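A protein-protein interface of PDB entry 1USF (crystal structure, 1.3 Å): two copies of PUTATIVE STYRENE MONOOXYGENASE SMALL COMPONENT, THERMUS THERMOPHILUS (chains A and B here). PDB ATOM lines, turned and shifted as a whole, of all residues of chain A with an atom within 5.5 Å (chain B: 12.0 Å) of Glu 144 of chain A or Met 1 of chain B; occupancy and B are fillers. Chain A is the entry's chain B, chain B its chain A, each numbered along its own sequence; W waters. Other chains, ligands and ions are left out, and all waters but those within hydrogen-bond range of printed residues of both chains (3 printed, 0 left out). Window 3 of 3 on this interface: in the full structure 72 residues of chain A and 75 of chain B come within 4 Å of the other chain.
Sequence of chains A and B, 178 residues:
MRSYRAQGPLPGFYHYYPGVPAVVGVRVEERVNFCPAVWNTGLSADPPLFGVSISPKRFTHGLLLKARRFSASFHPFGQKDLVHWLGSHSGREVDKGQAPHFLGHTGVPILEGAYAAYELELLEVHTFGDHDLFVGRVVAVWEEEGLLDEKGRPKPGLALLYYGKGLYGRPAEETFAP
No position is printed for both chains.
O of Ala 114 of chain A touches CE of Met 1 of chain B (3.3 Å). CE of Met 1 of chain B touches C of Tyr 115 of chain A, 3.9 Å away. CE1 of Tyr 115 of chain A touches O of His 15 of chain B, at 3.7 Å. Ala 116 of chain A touches Met 1 of chain B (N to CE, 3.8 Å). Ala 116 of chain A touches His 15 of chain B. CZ3 of Trp 142 of chain A touches O of Met 1 of chain B, 3.6 Å away. Trp 142 of chain A touches Arg 2 of chain B. Ser 3 of chain B touches Trp 142 of chain A. Glu 143 of chain A touches Met 1 of chain B (O to CG, 3.4 Å). Glu 144 of chain A touches Met 1 of chain B.
Water W3 lies within hydrogen-bond range of the side-chain hydroxyl of Tyr 115 of chain A (2.6 Å) and the backbone carbonyl oxygen of His 15 of chain B (2.7 Å). Water W1 lies within hydrogen-bond range of the side-chain carboxylate of Glu 143 of chain A (2.6 Å) and the side-chain hydroxyl of Tyr 4 of chain B (2.8 Å). Water W2 lies within hydrogen-bond range of N of Ala 114 of chain A (3.1 Å) and SD of Met 1 of chain B (3.7 Å).
Hydrophobic or aromatic side chains of chain B within 4 Å of the printed part of chain A: Met 1 and His 15. Of the 12 printed residues of chain A, 7 touch a printed residue of chain B. Hydrophobic or aromatic side chains of chain A that line the printed part of chain B: Tyr 115, Ala 116 and Trp 142. Among the printed residues, Asp or Glu carboxylates within 4 Å of a Lys or Arg side-chain nitrogen of the other chain: Glu 143 of chain A with Arg 2 of chain B.
Glu 144 of chain A touches just one residue of chain B: Met 1 (3.7 Å). Printed residues of chain B within 4 Å of Glu 145 of chain A: Arg 2. No residue of chain B comes within 4 Å of Leu 147 of chain A. No residue of chain B comes within 4 Å of Leu 148 of chain A. Printed residues of chain A within 4 Å of Ser 3 of chain B: Trp 142. Of the printed residues of chain A, Arg 2 of chain B touches Trp 142 (3.2 Å), Glu 143 (2.7 Å) and Glu 145 (2.8 Å). Printed residues of chain B within 4 Å of Tyr 115 of chain A: Met 1 and His 15. Of the printed residues of chain A, His 15 of chain B touches Tyr 115, Ala 116 and Glu 143. Gly 12 of chain B touches none of the printed residues of chain A. Tyr 16 of chain B touches none of the printed residues of chain A.
N of Trp 142 of chain A is in hydrogen-bond range of O of Ala 117 of chain A (2.9 Å). The backbone carbonyl oxygen (O) of Tyr 115 of chain A lies within hydrogen-bond range of the backbone NH (N) of Glu 144 of chain A (2.8 Å).
NE2 of His 15 of chain B lies within hydrogen-bond range of OE2 of Glu 143 of chain A (2.7 Å). The guanidinium group (NH1) of Arg 2 of chain B lies within salt-bridge range of the side-chain carboxylate (OE1) of Glu 143 of chain A, at 2.7 Å. The backbone NH (N) of Arg 2 of chain B lies close to the side-chain carboxylate (OE1) of Glu 145 of chain A, at 3.4 Å.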
ATOM      1  N   PHE A 102     -18.099  -2.904  35.762  1.00  0.00           N
ATOM      2  CA  PHE A 102     -18.640  -4.251  35.797  1.00  0.00           C
ATOM      3  C   PHE A 102     -17.458  -5.203  35.696  1.00  0.00           C
ATOM      4  O   PHE A 102     -16.347  -4.786  35.355  1.00  0.00           O
ATOM      5  CB  PHE A 102     -19.647  -4.468  34.652  1.00  0.00           C
ATOM      6  CG  PHE A 102     -19.041  -4.451  33.271  1.00  0.00           C
ATOM      7  CD1 PHE A 102     -18.550  -5.619  32.698  1.00  0.00           C
ATOM      8  CD2 PHE A 102     -19.000  -3.273  32.530  1.00  0.00           C
ATOM      9  CE1 PHE A 102     -18.032  -5.619  31.400  1.00  0.00           C
ATOM     10  CE2 PHE A 102     -18.483  -3.261  31.233  1.00  0.00           C
ATOM     11  CZ  PHE A 102     -18.000  -4.437  30.667  1.00  0.00           C
ATOM     12  N   ALA A 114     -17.386   2.692  28.239  1.00  0.00           N
ATOM     13  CA  ALA A 114     -16.433   2.505  27.149  1.00  0.00           C
ATOM     14  C   ALA A 114     -17.103   2.072  25.852  1.00  0.00           C
ATOM     15  O   ALA A 114     -18.165   1.445  25.872  1.00  0.00           O
ATOM     16  CB  ALA A 114     -15.396   1.469  27.550  1.00  0.00           C
ATOM     17  N   TYR A 115     -16.497   2.420  24.719  1.00  0.00           N
ATOM     18  CA  TYR A 115     -17.047   1.974  23.446  1.00  0.00           C
ATOM     19  C   TYR A 115     -16.402   0.630  23.115  1.00  0.00           C
ATOM     20  O   TYR A 115     -16.908  -0.124  22.291  1.00  0.00           O
ATOM     21  CB  TYR A 115     -16.825   3.006  22.322  1.00  0.00           C
ATOM     22  CG  TYR A 115     -15.438   3.606  22.204  1.00  0.00           C
ATOM     23  CD1 TYR A 115     -14.365   2.875  21.693  1.00  0.00           C
ATOM     24  CD2 TYR A 115     -15.209   4.927  22.586  1.00  0.00           C
ATOM     25  CE1 TYR A 115     -13.092   3.455  21.563  1.00  0.00           C
ATOM     26  CE2 TYR A 115     -13.952   5.510  22.463  1.00  0.00           C
ATOM     27  CZ  TYR A 115     -12.900   4.774  21.954  1.00  0.00           C
ATOM     28  OH  TYR A 115     -11.665   5.377  21.837  1.00  0.00           O
ATOM     29  N   ALA A 116     -15.301   0.318  23.793  1.00  0.00           N
ATOM     30  CA  ALA A 116     -14.605  -0.945  23.589  1.00  0.00           C
ATOM     31  C   ALA A 116     -13.655  -1.223  24.744  1.00  0.00           C
ATOM     32  O   ALA A 116     -13.199  -0.302  25.423  1.00  0.00           O
ATOM     33  CB  ALA A 116     -13.833  -0.921  22.273  1.00  0.00           C
ATOM     34  N   ALA A 117     -13.361  -2.495  24.974  1.00  0.00           N
ATOM     35  CA  ALA A 117     -12.446  -2.871  26.040  1.00  0.00           C
ATOM     36  C   ALA A 117     -11.888  -4.267  25.814  1.00  0.00           C
ATOM     37  O   ALA A 117     -12.514  -5.098  25.155  1.00  0.00           O
ATOM     38  CB  ALA A 117     -13.156  -2.804  27.394  1.00  0.00           C
ATOM     39  N   TRP A 142     -14.841  -6.553  24.322  1.00  0.00           N
ATOM     40  CA  TRP A 142     -16.130  -5.922  24.585  1.00  0.00           C
ATOM     41  C   TRP A 142     -16.302  -4.768  23.610  1.00  0.00           C
ATOM     42  O   TRP A 142     -15.365  -3.998  23.389  1.00  0.00           O
ATOM     43  CB  TRP A 142     -16.188  -5.384  26.016  1.00  0.00           C
ATOM     44  CG  TRP A 142     -16.208  -6.461  27.041  1.00  0.00           C
ATOM     45  CD1 TRP A 142     -15.142  -7.168  27.508  1.00  0.00           C
ATOM     46  CD2 TRP A 142     -17.365  -7.001  27.687  1.00  0.00           C
ATOM     47  NE1 TRP A 142     -15.562  -8.121  28.406  1.00  0.00           N
ATOM     48  CE2 TRP A 142     -16.924  -8.040  28.533  1.00  0.00           C
ATOM     49  CE3 TRP A 142     -18.734  -6.710  27.629  1.00  0.00           C
ATOM     50  CZ2 TRP A 142     -17.805  -8.791  29.323  1.00  0.00           C
ATOM     51  CZ3 TRP A 142     -19.610  -7.457  28.410  1.00  0.00           C
ATOM     52  CH2 TRP A 142     -19.139  -8.485  29.245  1.00  0.00           C
ATOM     53  N   GLU A 143     -17.491  -4.645  23.028  1.00  0.00           N
ATOM     54  CA  GLU A 143     -17.765  -3.581  22.069  1.00  0.00           C
ATOM     55  C   GLU A 143     -19.168  -3.012  22.240  1.00  0.00           C
ATOM     56  O   GLU A 143     -20.132  -3.760  22.419  1.00  0.00           O
ATOM     57  CB  GLU A 143     -17.639  -4.109  20.637  1.00  0.00           C
ATOM     58  CG  GLU A 143     -16.393  -4.928  20.359  1.00  0.00           C
ATOM     59  CD  GLU A 143     -16.335  -5.414  18.922  1.00  0.00           C
ATOM     60  OE1 GLU A 143     -17.389  -5.819  18.386  1.00  0.00           O
ATOM     61  OE2 GLU A 143     -15.240  -5.401  18.328  1.00  0.00           O
ATOM     62  N   GLU A 144     -19.283  -1.691  22.180  1.00  0.00           N
ATOM     63  CA  GLU A 144     -20.586  -1.047  22.285  1.00  0.00           C
ATOM     64  C   GLU A 144     -20.980  -0.744  20.839  1.00  0.00           C
ATOM     65  O   GLU A 144     -20.656   0.315  20.303  1.00  0.00           O
ATOM     66  CB  GLU A 144     -20.487   0.247  23.101  1.00  0.00           C
ATOM     67  CG  GLU A 144     -21.838   0.839  23.477  1.00  0.00           C
ATOM     68  CD  GLU A 144     -22.659  -0.090  24.352  1.00  0.00           C
ATOM     69  OE1 GLU A 144     -22.220  -0.389  25.483  1.00  0.00           O
ATOM     70  OE2 GLU A 144     -23.746  -0.522  23.909  1.00  0.00           O
ATOM     71  N   GLU A 145     -21.664  -1.700  20.214  1.00  0.00           N
ATOM     72  CA  GLU A 145     -22.095  -1.598  18.821  1.00  0.00           C
ATOM     73  C   GLU A 145     -22.464  -0.202  18.324  1.00  0.00           C
ATOM     74  O   GLU A 145     -21.973   0.243  17.286  1.00  0.00           O
ATOM     75  CB  GLU A 145     -23.285  -2.528  18.565  1.00  0.00           C
ATOM     76  CG  GLU A 145     -23.052  -3.993  18.894  1.00  0.00           C
ATOM     77  CD  GLU A 145     -23.298  -4.316  20.356  1.00  0.00           C
ATOM     78  OE1 GLU A 145     -23.415  -5.516  20.679  1.00  0.00           O
ATOM     79  OE2 GLU A 145     -23.376  -3.382  21.181  1.00  0.00           O
ATOM     80  N   GLY A 146     -23.334   0.479  19.060  1.00  0.00           N
ATOM     81  CA  GLY A 146     -23.766   1.806  18.657  1.00  0.00           C
ATOM     82  C   GLY A 146     -22.714   2.897  18.716  1.00  0.00           C
ATOM     83  O   GLY A 146     -22.993   4.046  18.370  1.00  0.00           O
ATOM     84  N   LEU A 147     -21.504   2.553  19.146  1.00  0.00           N
ATOM     85  CA  LEU A 147     -20.434   3.542  19.245  1.00  0.00           C
ATOM     86  C   LEU A 147     -19.213   3.187  18.402  1.00  0.00           C
ATOM     87  O   LEU A 147     -18.209   3.900  18.425  1.00  0.00           O
ATOM     88  CB  LEU A 147     -20.009   3.708  20.707  1.00  0.00           C
ATOM     89  CG  LEU A 147     -21.091   4.135  21.703  1.00  0.00           C
ATOM     90  CD1 LEU A 147     -20.501   4.178  23.106  1.00  0.00           C
ATOM     91  CD2 LEU A 147     -21.648   5.497  21.315  1.00  0.00           C
ATOM     92  N   LEU A 148     -19.299   2.092  17.653  1.00  0.00           N
ATOM     93  CA  LEU A 148     -18.181   1.661  16.821  1.00  0.00           C
ATOM     94  C   LEU A 148     -18.537   1.610  15.345  1.00  0.00           C
ATOM     95  O   LEU A 148     -19.705   1.441  14.987  1.00  0.00           O
ATOM     96  CB  LEU A 148     -17.699   0.276  17.258  1.00  0.00           C
ATOM     97  CG  LEU A 148     -17.204   0.117  18.696  1.00  0.00           C
ATOM     98  CD1 LEU A 148     -16.771  -1.322  18.928  1.00  0.00           C
ATOM     99  CD2 LEU A 148     -16.047   1.066  18.951  1.00  0.00           C
ATOM    100  N   MET B   1     -23.645  -4.403  26.073  1.00  0.00           N
ATOM    101  CA  MET B   1     -22.307  -4.331  25.418  1.00  0.00           C
ATOM    102  C   MET B   1     -21.917  -5.718  24.916  1.00  0.00           C
ATOM    103  O   MET B   1     -21.844  -6.672  25.693  1.00  0.00           O
ATOM    104  CB  MET B   1     -21.270  -3.813  26.422  1.00  0.00           C
ATOM    105  CG  MET B   1     -19.921  -3.443  25.823  1.00  0.00           C
ATOM    106  SD  MET B   1     -18.859  -2.572  27.008  1.00  0.00           S
ATOM    107  CE  MET B   1     -17.641  -1.823  25.890  1.00  0.00           C
ATOM    108  N   ARG B   2     -21.682  -5.830  23.612  1.00  0.00           N
ATOM    109  CA  ARG B   2     -21.299  -7.103  23.007  1.00  0.00           C
ATOM    110  C   ARG B   2     -19.957  -7.562  23.557  1.00  0.00           C
ATOM    111  O   ARG B   2     -19.100  -6.745  23.882  1.00  0.00           O
ATOM    112  CB  ARG B   2     -21.172  -6.964  21.487  1.00  0.00           C
ATOM    113  CG  ARG B   2     -20.698  -8.236  20.782  1.00  0.00           C
ATOM    114  CD  ARG B   2     -19.996  -7.932  19.460  1.00  0.00           C
ATOM    115  NE  ARG B   2     -19.631  -9.153  18.742  1.00  0.00           N
ATOM    116  CZ  ARG B   2     -18.818  -9.193  17.690  1.00  0.00           C
ATOM    117  NH1 ARG B   2     -18.272  -8.078  17.224  1.00  0.00           N
ATOM    118  NH2 ARG B   2     -18.555 -10.351  17.097  1.00  0.00           N
ATOM    119  N   SER B   3     -19.778  -8.873  23.659  1.00  0.00           N
ATOM    120  CA  SER B   3     -18.519  -9.421  24.133  1.00  0.00           C
ATOM    121  C   SER B   3     -18.300 -10.784  23.501  1.00  0.00           C
ATOM    122  O   SER B   3     -19.253 -11.491  23.174  1.00  0.00           O
ATOM    123  CB  SER B   3     -18.510  -9.556  25.658  1.00  0.00           C
ATOM    124  OG  SER B   3     -19.280 -10.664  26.090  1.00  0.00           O
ATOM    125  N   TYR B   4     -17.038 -11.136  23.304  1.00  0.00           N
ATOM    126  CA  TYR B   4     -16.706 -12.431  22.741  1.00  0.00           C
ATOM    127  C   TYR B   4     -15.323 -12.853  23.199  1.00  0.00           C
ATOM    128  O   TYR B   4     -14.498 -12.021  23.587  1.00  0.00           O
ATOM    129  CB  TYR B   4     -16.811 -12.412  21.203  1.00  0.00           C
ATOM    130  CG  TYR B   4     -15.803 -11.547  20.469  1.00  0.00           C
ATOM    131  CD1 TYR B   4     -14.516 -12.017  20.193  1.00  0.00           C
ATOM    132  CD2 TYR B   4     -16.147 -10.272  20.024  1.00  0.00           C
ATOM    133  CE1 TYR B   4     -13.598 -11.237  19.490  1.00  0.00           C
ATOM    134  CE2 TYR B   4     -15.238  -9.481  19.320  1.00  0.00           C
ATOM    135  CZ  TYR B   4     -13.966  -9.972  19.056  1.00  0.00           C
ATOM    136  OH  TYR B   4     -13.065  -9.197  18.357  1.00  0.00           O
ATOM    137  N   ARG B   5     -15.093 -14.159  23.186  1.00  0.00           N
ATOM    138  CA  ARG B   5     -13.826 -14.741  23.592  1.00  0.00           C
ATOM    139  C   ARG B   5     -12.823 -14.638  22.450  1.00  0.00           C
ATOM    140  O   ARG B   5     -13.155 -14.932  21.303  1.00  0.00           O
ATOM    141  CB  ARG B   5     -14.041 -16.215  23.947  1.00  0.00           C
ATOM    142  CG  ARG B   5     -12.782 -16.989  24.296  1.00  0.00           C
ATOM    143  CD  ARG B   5     -13.072 -18.488  24.313  1.00  0.00           C
ATOM    144  NE  ARG B   5     -14.124 -18.840  25.264  1.00  0.00           N
ATOM    145  CZ  ARG B   5     -13.942 -18.965  26.576  1.00  0.00           C
ATOM    146  NH1 ARG B   5     -14.964 -19.285  27.359  1.00  0.00           N
ATOM    147  NH2 ARG B   5     -12.739 -18.789  27.104  1.00  0.00           N
ATOM    148  N   GLY B  12     -10.762  -7.306  13.616  1.00  0.00           N
ATOM    149  CA  GLY B  12     -10.220  -5.973  13.434  1.00  0.00           C
ATOM    150  C   GLY B  12      -9.615  -5.585  14.770  1.00  0.00           C
ATOM    151  O   GLY B  12     -10.326  -5.501  15.767  1.00  0.00           O
ATOM    152  N   TYR B  14      -8.486  -2.754  16.082  1.00  0.00           N
ATOM    153  CA  TYR B  14      -8.438  -1.291  16.045  1.00  0.00           C
ATOM    154  C   TYR B  14      -9.171  -0.566  17.162  1.00  0.00           C
ATOM    155  O   TYR B  14      -9.392   0.643  17.070  1.00  0.00           O
ATOM    156  CB  TYR B  14      -9.012  -0.805  14.709  1.00  0.00           C
ATOM    157  CG  TYR B  14      -8.352  -1.426  13.509  1.00  0.00           C
ATOM    158  CD1 TYR B  14      -9.029  -2.348  12.708  1.00  0.00           C
ATOM    159  CD2 TYR B  14      -7.034  -1.117  13.191  1.00  0.00           C
ATOM    160  CE1 TYR B  14      -8.400  -2.949  11.618  1.00  0.00           C
ATOM    161  CE2 TYR B  14      -6.397  -1.706  12.112  1.00  0.00           C
ATOM    162  CZ  TYR B  14      -7.082  -2.620  11.331  1.00  0.00           C
ATOM    163  OH  TYR B  14      -6.435  -3.201  10.269  1.00  0.00           O
ATOM    164  N   HIS B  15      -9.531  -1.280  18.217  1.00  0.00           N
ATOM    165  CA  HIS B  15     -10.281  -0.671  19.311  1.00  0.00           C
ATOM    166  C   HIS B  15      -9.585   0.475  20.025  1.00  0.00           C
ATOM    167  O   HIS B  15     -10.250   1.343  20.593  1.00  0.00           O
ATOM    168  CB  HIS B  15     -10.676  -1.737  20.328  1.00  0.00           C
ATOM    169  CG  HIS B  15     -11.395  -2.894  19.720  1.00  0.00           C
ATOM    170  ND1 HIS B  15     -10.741  -3.899  19.043  1.00  0.00           N
ATOM    171  CD2 HIS B  15     -12.717  -3.178  19.633  1.00  0.00           C
ATOM    172  CE1 HIS B  15     -11.628  -4.753  18.565  1.00  0.00           C
ATOM    173  NE2 HIS B  15     -12.833  -4.338  18.907  1.00  0.00           N
ATOM    174  N   TYR B  16      -8.258   0.466  19.997  1.00  0.00           N
ATOM    175  CA  TYR B  16      -7.454   1.492  20.654  1.00  0.00           C
ATOM    176  C   TYR B  16      -6.963   2.583  19.694  1.00  0.00           C
ATOM    177  O   TYR B  16      -6.139   3.423  20.073  1.00  0.00           O
ATOM    178  CB  TYR B  16      -6.257   0.843  21.353  1.00  0.00           C
ATOM    179  CG  TYR B  16      -5.474  -0.073  20.446  1.00  0.00           C
ATOM    180  CD1 TYR B  16      -5.896  -1.380  20.215  1.00  0.00           C
ATOM    181  CD2 TYR B  16      -4.334   0.380  19.786  1.00  0.00           C
ATOM    182  CE1 TYR B  16      -5.204  -2.215  19.344  1.00  0.00           C
ATOM    183  CE2 TYR B  16      -3.636  -0.443  18.915  1.00  0.00           C
ATOM    184  CZ  TYR B  16      -4.078  -1.738  18.697  1.00  0.00           C
ATOM    185  OH  TYR B  16      -3.402  -2.550  17.822  1.00  0.00           O
HETATM  186  O   HOH W   1     -14.478  -7.347  16.799  1.00  0.00           O
HETATM  187  O   HOH W   2     -17.638  -0.145  29.492  1.00  0.00           O
HETATM  188  O   HOH W   3      -9.786   4.016  20.760  1.00  0.00           O
